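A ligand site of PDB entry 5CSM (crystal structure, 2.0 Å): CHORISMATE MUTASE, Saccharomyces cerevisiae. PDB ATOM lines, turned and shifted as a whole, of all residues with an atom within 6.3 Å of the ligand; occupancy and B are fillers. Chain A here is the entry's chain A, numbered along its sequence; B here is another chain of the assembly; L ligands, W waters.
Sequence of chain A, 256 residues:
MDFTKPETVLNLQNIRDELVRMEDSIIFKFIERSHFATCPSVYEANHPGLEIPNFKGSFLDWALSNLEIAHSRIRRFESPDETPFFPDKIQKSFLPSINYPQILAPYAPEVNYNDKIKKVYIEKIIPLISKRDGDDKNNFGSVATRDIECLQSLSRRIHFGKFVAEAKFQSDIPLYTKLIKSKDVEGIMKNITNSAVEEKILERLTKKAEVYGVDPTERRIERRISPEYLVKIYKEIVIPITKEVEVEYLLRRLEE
Residues that only touch the ligand: Arg 76 of chain B (3.4 Å), Thr 145 (3.6 Å), Ile 74 of chain B (3.7 Å), His 71 of chain B (3.8 Å) and Glu 82 of chain B (3.96 Å). The nearest printed residue that does not touch the ligand is Ser 79 of chain B (4.0005 Å).
Water W3 lies within hydrogen-bond range of N2 of the ligand (2.8 Å), OG1 of Thr 145 (3.3 Å) and NH1 of Arg 146 (3.5 Å). Water W4 lies within hydrogen-bond range of a nitrogen (N1) of the ligand and the side-chain carboxylate (OD2) of Asp 81 of chain B. Water W1 lies within hydrogen-bond range of an oxygen (O1) of the ligand (2.8 Å), the backbone carbonyl oxygen (O) of Arg 75 of chain B (2.9 Å) and the side-chain hydroxyl (OH) of Tyr 100 of chain B (2.9 Å). Water W2 lies within hydrogen-bond range of the guanidinium group of Arg 75 of chain B (2.9 Å), an oxygen (O1) of the ligand (2.9 Å) and the backbone carbonyl oxygen of Ile 74 of chain B (3.0 Å). Water W5 lies within hydrogen-bond range of O of Lys 137 (2.9 Å), O1 of the ligand (3.0 Å), N of Phe 140 (3.0 Å) and NH2 of Arg 75 of chain B (3.4 Å).
The backbone NH of Gly 141 is in hydrogen-bond range of an oxygen (O2) of the ligand. O of Asn 138 sits close to N1 of the ligand, at 3.3 Å. N1 of the ligand sits at hydrogen-bond distance from OG of Ser 142 (3.0 Å). N1 of the ligand sits at hydrogen-bond distance from OD1 of Asn 139. The backbone NH of Phe 140 lies within hydrogen-bond range of an oxygen (O2) of the ligand (3.4 Å). The backbone NH (N) of Ser 142 sits at hydrogen-bond distance from an oxygen (O2) of the ligand.
The guanidinium group (NE) of Arg 76 of chain B is in salt-bridge range of the side-chain carboxylate (OE1) of Glu 82 of chain B (3.0 Å). The guanidinium group (NH1) of Arg 146 sits at hydrogen-bond distance from the backbone carbonyl oxygen (O) of Ser 142 (3.0 Å). O of Gly 141 lies close to OG1 of Thr 145, at 3.3 Å. O of Ser 142 sits at hydrogen-bond distance from OG1 of Thr 145 (3.2 Å). OG of Ser 142 is in hydrogen-bond range of OD1 of Asn 139, at 3.5 Å. A ring nitrogen (ND1) of His 71 of chain B lies within hydrogen-bond range of the guanidinium group (NH1) of Arg 76 of chain B.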
ATOM      1  N   PHE A  59       2.375  -8.325  -3.951  1.00  0.00           N
ATOM      2  CA  PHE A  59       2.507  -7.955  -2.547  1.00  0.00           C
ATOM      3  C   PHE A  59       1.201  -7.247  -2.150  1.00  0.00           C
ATOM      4  O   PHE A  59       0.706  -7.398  -1.015  1.00  0.00           O
ATOM      5  CB  PHE A  59       3.742  -7.032  -2.401  1.00  0.00           C
ATOM      6  CG  PHE A  59       4.112  -6.687  -0.974  1.00  0.00           C
ATOM      7  CD1 PHE A  59       4.646  -7.657  -0.127  1.00  0.00           C
ATOM      8  CD2 PHE A  59       4.050  -5.385  -0.520  1.00  0.00           C
ATOM      9  CE1 PHE A  59       5.111  -7.308   1.150  1.00  0.00           C
ATOM     10  CE2 PHE A  59       4.515  -5.037   0.757  1.00  0.00           C
ATOM     11  CZ  PHE A  59       5.043  -5.990   1.579  1.00  0.00           C
ATOM     12  N   LYS A 137      12.543   0.828  -2.064  1.00  0.00           N
ATOM     13  CA  LYS A 137      12.767  -0.433  -1.387  1.00  0.00           C
ATOM     14  C   LYS A 137      12.462  -0.477   0.098  1.00  0.00           C
ATOM     15  O   LYS A 137      12.224  -1.548   0.648  1.00  0.00           O
ATOM     16  CB  LYS A 137      14.237  -0.838  -1.586  1.00  0.00           C
ATOM     17  CG  LYS A 137      14.503  -2.027  -2.511  1.00  0.00           C
ATOM     18  CD  LYS A 137      14.071  -1.768  -3.946  1.00  0.00           C
ATOM     19  CE  LYS A 137      14.269  -3.036  -4.817  1.00  0.00           C
ATOM     20  NZ  LYS A 137      13.765  -2.936  -6.253  1.00  0.00           N
ATOM     21  N   ASN A 138      12.536   0.671   0.774  1.00  0.00           N
ATOM     22  CA  ASN A 138      12.304   0.708   2.217  1.00  0.00           C
ATOM     23  C   ASN A 138      10.879   1.097   2.601  1.00  0.00           C
ATOM     24  O   ASN A 138      10.600   1.269   3.779  1.00  0.00           O
ATOM     25  CB  ASN A 138      13.246   1.728   2.861  1.00  0.00           C
ATOM     26  CG  ASN A 138      14.697   1.565   2.422  1.00  0.00           C
ATOM     27  OD1 ASN A 138      15.348   2.547   2.085  1.00  0.00           O
ATOM     28  ND2 ASN A 138      15.191   0.326   2.408  1.00  0.00           N
ATOM     29  N   ASN A 139      10.042   1.349   1.591  1.00  0.00           N
ATOM     30  CA  ASN A 139       8.650   1.746   1.815  1.00  0.00           C
ATOM     31  C   ASN A 139       7.573   0.918   1.113  1.00  0.00           C
ATOM     32  O   ASN A 139       6.453   1.404   0.934  1.00  0.00           O
ATOM     33  CB  ASN A 139       8.436   3.226   1.470  1.00  0.00           C
ATOM     34  CG  ASN A 139       8.963   4.157   2.537  1.00  0.00           C
ATOM     35  OD1 ASN A 139       8.498   4.109   3.667  1.00  0.00           O
ATOM     36  ND2 ASN A 139       9.880   5.026   2.171  1.00  0.00           N
ATOM     37  N   PHE A 140       7.880  -0.333   0.769  1.00  0.00           N
ATOM     38  CA  PHE A 140       6.904  -1.202   0.136  1.00  0.00           C
ATOM     39  C   PHE A 140       5.635  -1.425   0.969  1.00  0.00           C
ATOM     40  O   PHE A 140       4.531  -1.391   0.446  1.00  0.00           O
ATOM     41  CB  PHE A 140       7.531  -2.520  -0.301  1.00  0.00           C
ATOM     42  CG  PHE A 140       8.470  -2.395  -1.475  1.00  0.00           C
ATOM     43  CD1 PHE A 140       8.343  -1.338  -2.389  1.00  0.00           C
ATOM     44  CD2 PHE A 140       9.444  -3.373  -1.716  1.00  0.00           C
ATOM     45  CE1 PHE A 140       9.164  -1.244  -3.501  1.00  0.00           C
ATOM     46  CE2 PHE A 140      10.272  -3.291  -2.844  1.00  0.00           C
ATOM     47  CZ  PHE A 140      10.128  -2.223  -3.744  1.00  0.00           C
ATOM     48  N   GLY A 141       5.807  -1.650   2.267  1.00  0.00           N
ATOM     49  CA  GLY A 141       4.661  -1.846   3.135  1.00  0.00           C
ATOM     50  C   GLY A 141       3.884  -0.563   3.383  1.00  0.00           C
ATOM     51  O   GLY A 141       2.661  -0.616   3.500  1.00  0.00           O
ATOM     52  N   SER A 142       4.575   0.570   3.564  1.00  0.00           N
ATOM     53  CA  SER A 142       3.905   1.864   3.760  1.00  0.00           C
ATOM     54  C   SER A 142       3.021   2.172   2.559  1.00  0.00           C
ATOM     55  O   SER A 142       1.909   2.683   2.705  1.00  0.00           O
ATOM     56  CB  SER A 142       4.910   2.991   3.912  1.00  0.00           C
ATOM     57  OG  SER A 142       5.591   2.883   5.139  1.00  0.00           O
ATOM     58  N   VAL A 143       3.541   1.888   1.365  1.00  0.00           N
ATOM     59  CA  VAL A 143       2.788   2.104   0.154  1.00  0.00           C
ATOM     60  C   VAL A 143       1.560   1.203   0.081  1.00  0.00           C
ATOM     61  O   VAL A 143       0.457   1.709  -0.055  1.00  0.00           O
ATOM     62  CB  VAL A 143       3.689   1.923  -1.064  1.00  0.00           C
ATOM     63  CG1 VAL A 143       2.866   1.749  -2.316  1.00  0.00           C
ATOM     64  CG2 VAL A 143       4.552   3.161  -1.203  1.00  0.00           C
ATOM     65  N   THR A 145      -0.226  -0.333   2.298  1.00  0.00           N
ATOM     66  CA  THR A 145      -1.283  -0.021   3.228  1.00  0.00           C
ATOM     67  C   THR A 145      -2.023   1.260   2.834  1.00  0.00           C
ATOM     68  O   THR A 145      -3.228   1.394   3.089  1.00  0.00           O
ATOM     69  CB  THR A 145      -0.772   0.040   4.707  1.00  0.00           C
ATOM     70  OG1 THR A 145       0.165   1.101   4.869  1.00  0.00           O
ATOM     71  CG2 THR A 145      -0.115  -1.277   5.113  1.00  0.00           C
ATOM     72  N   ARG A 146      -1.319   2.210   2.222  1.00  0.00           N
ATOM     73  CA  ARG A 146      -1.926   3.459   1.746  1.00  0.00           C
ATOM     74  C   ARG A 146      -2.788   3.090   0.508  1.00  0.00           C
ATOM     75  O   ARG A 146      -3.815   3.689   0.279  1.00  0.00           O
ATOM     76  CB  ARG A 146      -0.885   4.524   1.327  1.00  0.00           C
ATOM     77  CG  ARG A 146       0.076   5.076   2.390  1.00  0.00           C
ATOM     78  CD  ARG A 146      -0.632   5.548   3.595  1.00  0.00           C
ATOM     79  NE  ARG A 146       0.248   6.331   4.496  1.00  0.00           N
ATOM     80  CZ  ARG A 146       1.350   5.901   5.147  1.00  0.00           C
ATOM     81  NH1 ARG A 146       1.822   4.666   4.989  1.00  0.00           N
ATOM     82  NH2 ARG A 146       2.001   6.745   5.937  1.00  0.00           N
ATOM     83  N   HIS B  71       1.201  -7.596   9.697  1.00  0.00           N
ATOM     84  CA  HIS B  71       2.219  -6.637   9.265  1.00  0.00           C
ATOM     85  C   HIS B  71       3.630  -6.990   9.716  1.00  0.00           C
ATOM     86  O   HIS B  71       4.571  -6.711   8.974  1.00  0.00           O
ATOM     87  CB  HIS B  71       1.882  -5.197   9.658  1.00  0.00           C
ATOM     88  CG  HIS B  71       0.727  -4.608   8.894  1.00  0.00           C
ATOM     89  ND1 HIS B  71       0.266  -3.333   9.103  1.00  0.00           N
ATOM     90  CD2 HIS B  71      -0.035  -5.112   7.885  1.00  0.00           C
ATOM     91  CE1 HIS B  71      -0.718  -3.065   8.267  1.00  0.00           C
ATOM     92  NE2 HIS B  71      -0.917  -4.127   7.509  1.00  0.00           N
ATOM     93  N   SER B  72       3.778  -7.647  10.876  1.00  0.00           N
ATOM     94  CA  SER B  72       5.098  -8.061  11.382  1.00  0.00           C
ATOM     95  C   SER B  72       5.725  -9.097  10.441  1.00  0.00           C
ATOM     96  O   SER B  72       6.938  -9.095  10.202  1.00  0.00           O
ATOM     97  CB  SER B  72       5.017  -8.648  12.789  1.00  0.00           C
ATOM     98  OG  SER B  72       4.444  -9.937  12.823  1.00  0.00           O
ATOM     99  N   ILE B  74       5.438  -9.059   7.298  1.00  0.00           N
ATOM    100  CA  ILE B  74       5.969  -8.345   6.159  1.00  0.00           C
ATOM    101  C   ILE B  74       6.969  -7.216   6.510  1.00  0.00           C
ATOM    102  O   ILE B  74       7.150  -6.293   5.720  1.00  0.00           O
ATOM    103  CB  ILE B  74       4.911  -7.888   5.158  1.00  0.00           C
ATOM    104  CG1 ILE B  74       3.803  -7.092   5.847  1.00  0.00           C
ATOM    105  CG2 ILE B  74       4.406  -9.095   4.368  1.00  0.00           C
ATOM    106  CD1 ILE B  74       2.832  -6.505   4.844  1.00  0.00           C
ATOM    107  N   ARG B  75       7.638  -7.326   7.670  1.00  0.00           N
ATOM    108  CA  ARG B  75       8.698  -6.422   8.103  1.00  0.00           C
ATOM    109  C   ARG B  75       8.375  -5.059   8.701  1.00  0.00           C
ATOM    110  O   ARG B  75       9.273  -4.222   8.819  1.00  0.00           O
ATOM    111  CB  ARG B  75       9.702  -6.214   6.958  1.00  0.00           C
ATOM    112  CG  ARG B  75      10.224  -7.500   6.284  1.00  0.00           C
ATOM    113  CD  ARG B  75      11.167  -7.224   5.100  1.00  0.00           C
ATOM    114  NE  ARG B  75      10.524  -6.395   4.080  1.00  0.00           N
ATOM    115  CZ  ARG B  75      10.927  -6.314   2.821  1.00  0.00           C
ATOM    116  NH1 ARG B  75      11.991  -7.005   2.420  1.00  0.00           N
ATOM    117  NH2 ARG B  75      10.281  -5.523   1.943  1.00  0.00           N
ATOM    118  N   ARG B  76       7.143  -4.829   9.113  1.00  0.00           N
ATOM    119  CA  ARG B  76       6.781  -3.520   9.654  1.00  0.00           C
ATOM    120  C   ARG B  76       7.644  -3.067  10.849  1.00  0.00           C
ATOM    121  O   ARG B  76       8.177  -1.957  10.858  1.00  0.00           O
ATOM    122  CB  ARG B  76       5.294  -3.507  10.071  1.00  0.00           C
ATOM    123  CG  ARG B  76       4.812  -2.104  10.509  1.00  0.00           C
ATOM    124  CD  ARG B  76       3.304  -1.972  10.798  1.00  0.00           C
ATOM    125  NE  ARG B  76       3.038  -0.562  11.101  1.00  0.00           N
ATOM    126  CZ  ARG B  76       2.011   0.150  10.634  1.00  0.00           C
ATOM    127  NH1 ARG B  76       1.087  -0.416   9.890  1.00  0.00           N
ATOM    128  NH2 ARG B  76       1.883   1.426  10.966  1.00  0.00           N
ATOM    129  N   PHE B  77       7.779  -3.915  11.852  1.00  0.00           N
ATOM    130  CA  PHE B  77       8.519  -3.573  13.056  1.00  0.00           C
ATOM    131  C   PHE B  77      10.039  -3.727  12.995  1.00  0.00           C
ATOM    132  O   PHE B  77      10.698  -3.647  14.021  1.00  0.00           O
ATOM    133  CB  PHE B  77       7.875  -4.250  14.239  1.00  0.00           C
ATOM    134  CG  PHE B  77       6.431  -3.874  14.366  1.00  0.00           C
ATOM    135  CD1 PHE B  77       6.077  -2.555  14.655  1.00  0.00           C
ATOM    136  CD2 PHE B  77       5.422  -4.788  14.087  1.00  0.00           C
ATOM    137  CE1 PHE B  77       4.752  -2.151  14.645  1.00  0.00           C
ATOM    138  CE2 PHE B  77       4.069  -4.398  14.071  1.00  0.00           C
ATOM    139  CZ  PHE B  77       3.740  -3.069  14.345  1.00  0.00           C
ATOM    140  N   SER B  79      11.497  -1.730  11.035  1.00  0.00           N
ATOM    141  CA  SER B  79      11.850  -0.331  10.801  1.00  0.00           C
ATOM    142  C   SER B  79      11.917   0.389  12.147  1.00  0.00           C
ATOM    143  O   SER B  79      11.032   0.211  12.976  1.00  0.00           O
ATOM    144  CB  SER B  79      10.845   0.328   9.884  1.00  0.00           C
ATOM    145  OG  SER B  79      11.318   1.621   9.502  1.00  0.00           O
ATOM    146  N   ASP B  81      11.285   3.442  13.101  1.00  0.00           N
ATOM    147  CA  ASP B  81      10.190   4.376  13.384  1.00  0.00           C
ATOM    148  C   ASP B  81       8.847   3.719  13.738  1.00  0.00           C
ATOM    149  O   ASP B  81       7.887   4.440  14.019  1.00  0.00           O
ATOM    150  CB  ASP B  81       9.993   5.341  12.208  1.00  0.00           C
ATOM    151  CG  ASP B  81       9.680   4.645  10.900  1.00  0.00           C
ATOM    152  OD1 ASP B  81      10.086   3.485  10.679  1.00  0.00           O
ATOM    153  OD2 ASP B  81       9.044   5.290  10.056  1.00  0.00           O
ATOM    154  N   GLU B  82       8.775   2.393  13.763  1.00  0.00           N
ATOM    155  CA  GLU B  82       7.526   1.696  14.067  1.00  0.00           C
ATOM    156  C   GLU B  82       7.651   0.975  15.408  1.00  0.00           C
ATOM    157  O   GLU B  82       8.531   0.123  15.544  1.00  0.00           O
ATOM    158  CB  GLU B  82       7.214   0.676  12.951  1.00  0.00           C
ATOM    159  CG  GLU B  82       7.018   1.269  11.553  1.00  0.00           C
ATOM    160  CD  GLU B  82       5.768   2.110  11.432  1.00  0.00           C
ATOM    161  OE1 GLU B  82       4.754   1.740  12.037  1.00  0.00           O
ATOM    162  OE2 GLU B  82       5.781   3.160  10.763  1.00  0.00           O
ATOM    163  N   ILE B  98      15.437  -6.337   5.772  1.00  0.00           N
ATOM    164  CA  ILE B  98      16.082  -5.138   5.276  1.00  0.00           C
ATOM    165  C   ILE B  98      17.141  -4.884   6.326  1.00  0.00           C
ATOM    166  O   ILE B  98      16.857  -5.016   7.524  1.00  0.00           O
ATOM    167  CB  ILE B  98      15.090  -3.951   5.260  1.00  0.00           C
ATOM    168  CG1 ILE B  98      13.905  -4.279   4.319  1.00  0.00           C
ATOM    169  CG2 ILE B  98      15.830  -2.665   4.866  1.00  0.00           C
ATOM    170  CD1 ILE B  98      12.751  -3.303   4.346  1.00  0.00           C
ATOM    171  N   TYR B 100      18.859  -2.540   8.366  1.00  0.00           N
ATOM    172  CA  TYR B 100      18.843  -1.178   8.847  1.00  0.00           C
ATOM    173  C   TYR B 100      20.072  -0.958   9.722  1.00  0.00           C
ATOM    174  O   TYR B 100      20.310  -1.726  10.661  1.00  0.00           O
ATOM    175  CB  TYR B 100      17.577  -0.964   9.674  1.00  0.00           C
ATOM    176  CG  TYR B 100      16.299  -0.912   8.872  1.00  0.00           C
ATOM    177  CD1 TYR B 100      16.080   0.141   7.984  1.00  0.00           C
ATOM    178  CD2 TYR B 100      15.302  -1.887   9.018  1.00  0.00           C
ATOM    179  CE1 TYR B 100      14.896   0.247   7.267  1.00  0.00           C
ATOM    180  CE2 TYR B 100      14.109  -1.792   8.300  1.00  0.00           C
ATOM    181  CZ  TYR B 100      13.925  -0.723   7.431  1.00  0.00           C
ATOM    182  OH  TYR B 100      12.757  -0.585   6.715  1.00  0.00           O
HETATM  183  N1  LIG L   1       8.144   1.621   5.972  1.00  0.00           N
HETATM  184  C1  LIG L   1       8.493   0.204   6.255  1.00  0.00           C
HETATM  185  C2  LIG L   1       8.245  -0.647   5.020  1.00  0.00           C
HETATM  186  O1  LIG L   1       8.759  -1.781   4.955  1.00  0.00           O
HETATM  187  C3  LIG L   1       7.725  -0.307   7.462  1.00  0.00           C
HETATM  188  C4  LIG L   1       6.232  -0.292   7.349  1.00  0.00           C
HETATM  189  C5  LIG L   1       5.410   0.733   7.661  1.00  0.00           C
HETATM  190  C6  LIG L   1       5.377  -1.397   6.997  1.00  0.00           C
HETATM  191  N2  LIG L   1       4.101   0.347   7.545  1.00  0.00           N
HETATM  192  C7  LIG L   1       4.047  -0.949   7.127  1.00  0.00           C
HETATM  193  C8  LIG L   1       5.595  -2.717   6.593  1.00  0.00           C
HETATM  194  C9  LIG L   1       2.955  -1.766   6.873  1.00  0.00           C
HETATM  195  C10 LIG L   1       4.501  -3.542   6.350  1.00  0.00           C
HETATM  196  C11 LIG L   1       3.203  -3.048   6.494  1.00  0.00           C
HETATM  197  O2  LIG L   1       7.532  -0.171   4.123  1.00  0.00           O
HETATM  198  O   HOH W   1      10.634  -2.569   6.928  1.00  0.00           O
HETATM  199  O   HOH W   2       8.340  -4.393   3.754  1.00  0.00           O
HETATM  200  O   HOH W   3       1.998   2.168   7.426  1.00  0.00           O
HETATM  201  O   HOH W   4       8.039   3.454   8.102  1.00  0.00           O
HETATM  202  O   HOH W   5       9.852  -2.172   2.190  1.00  0.00           O
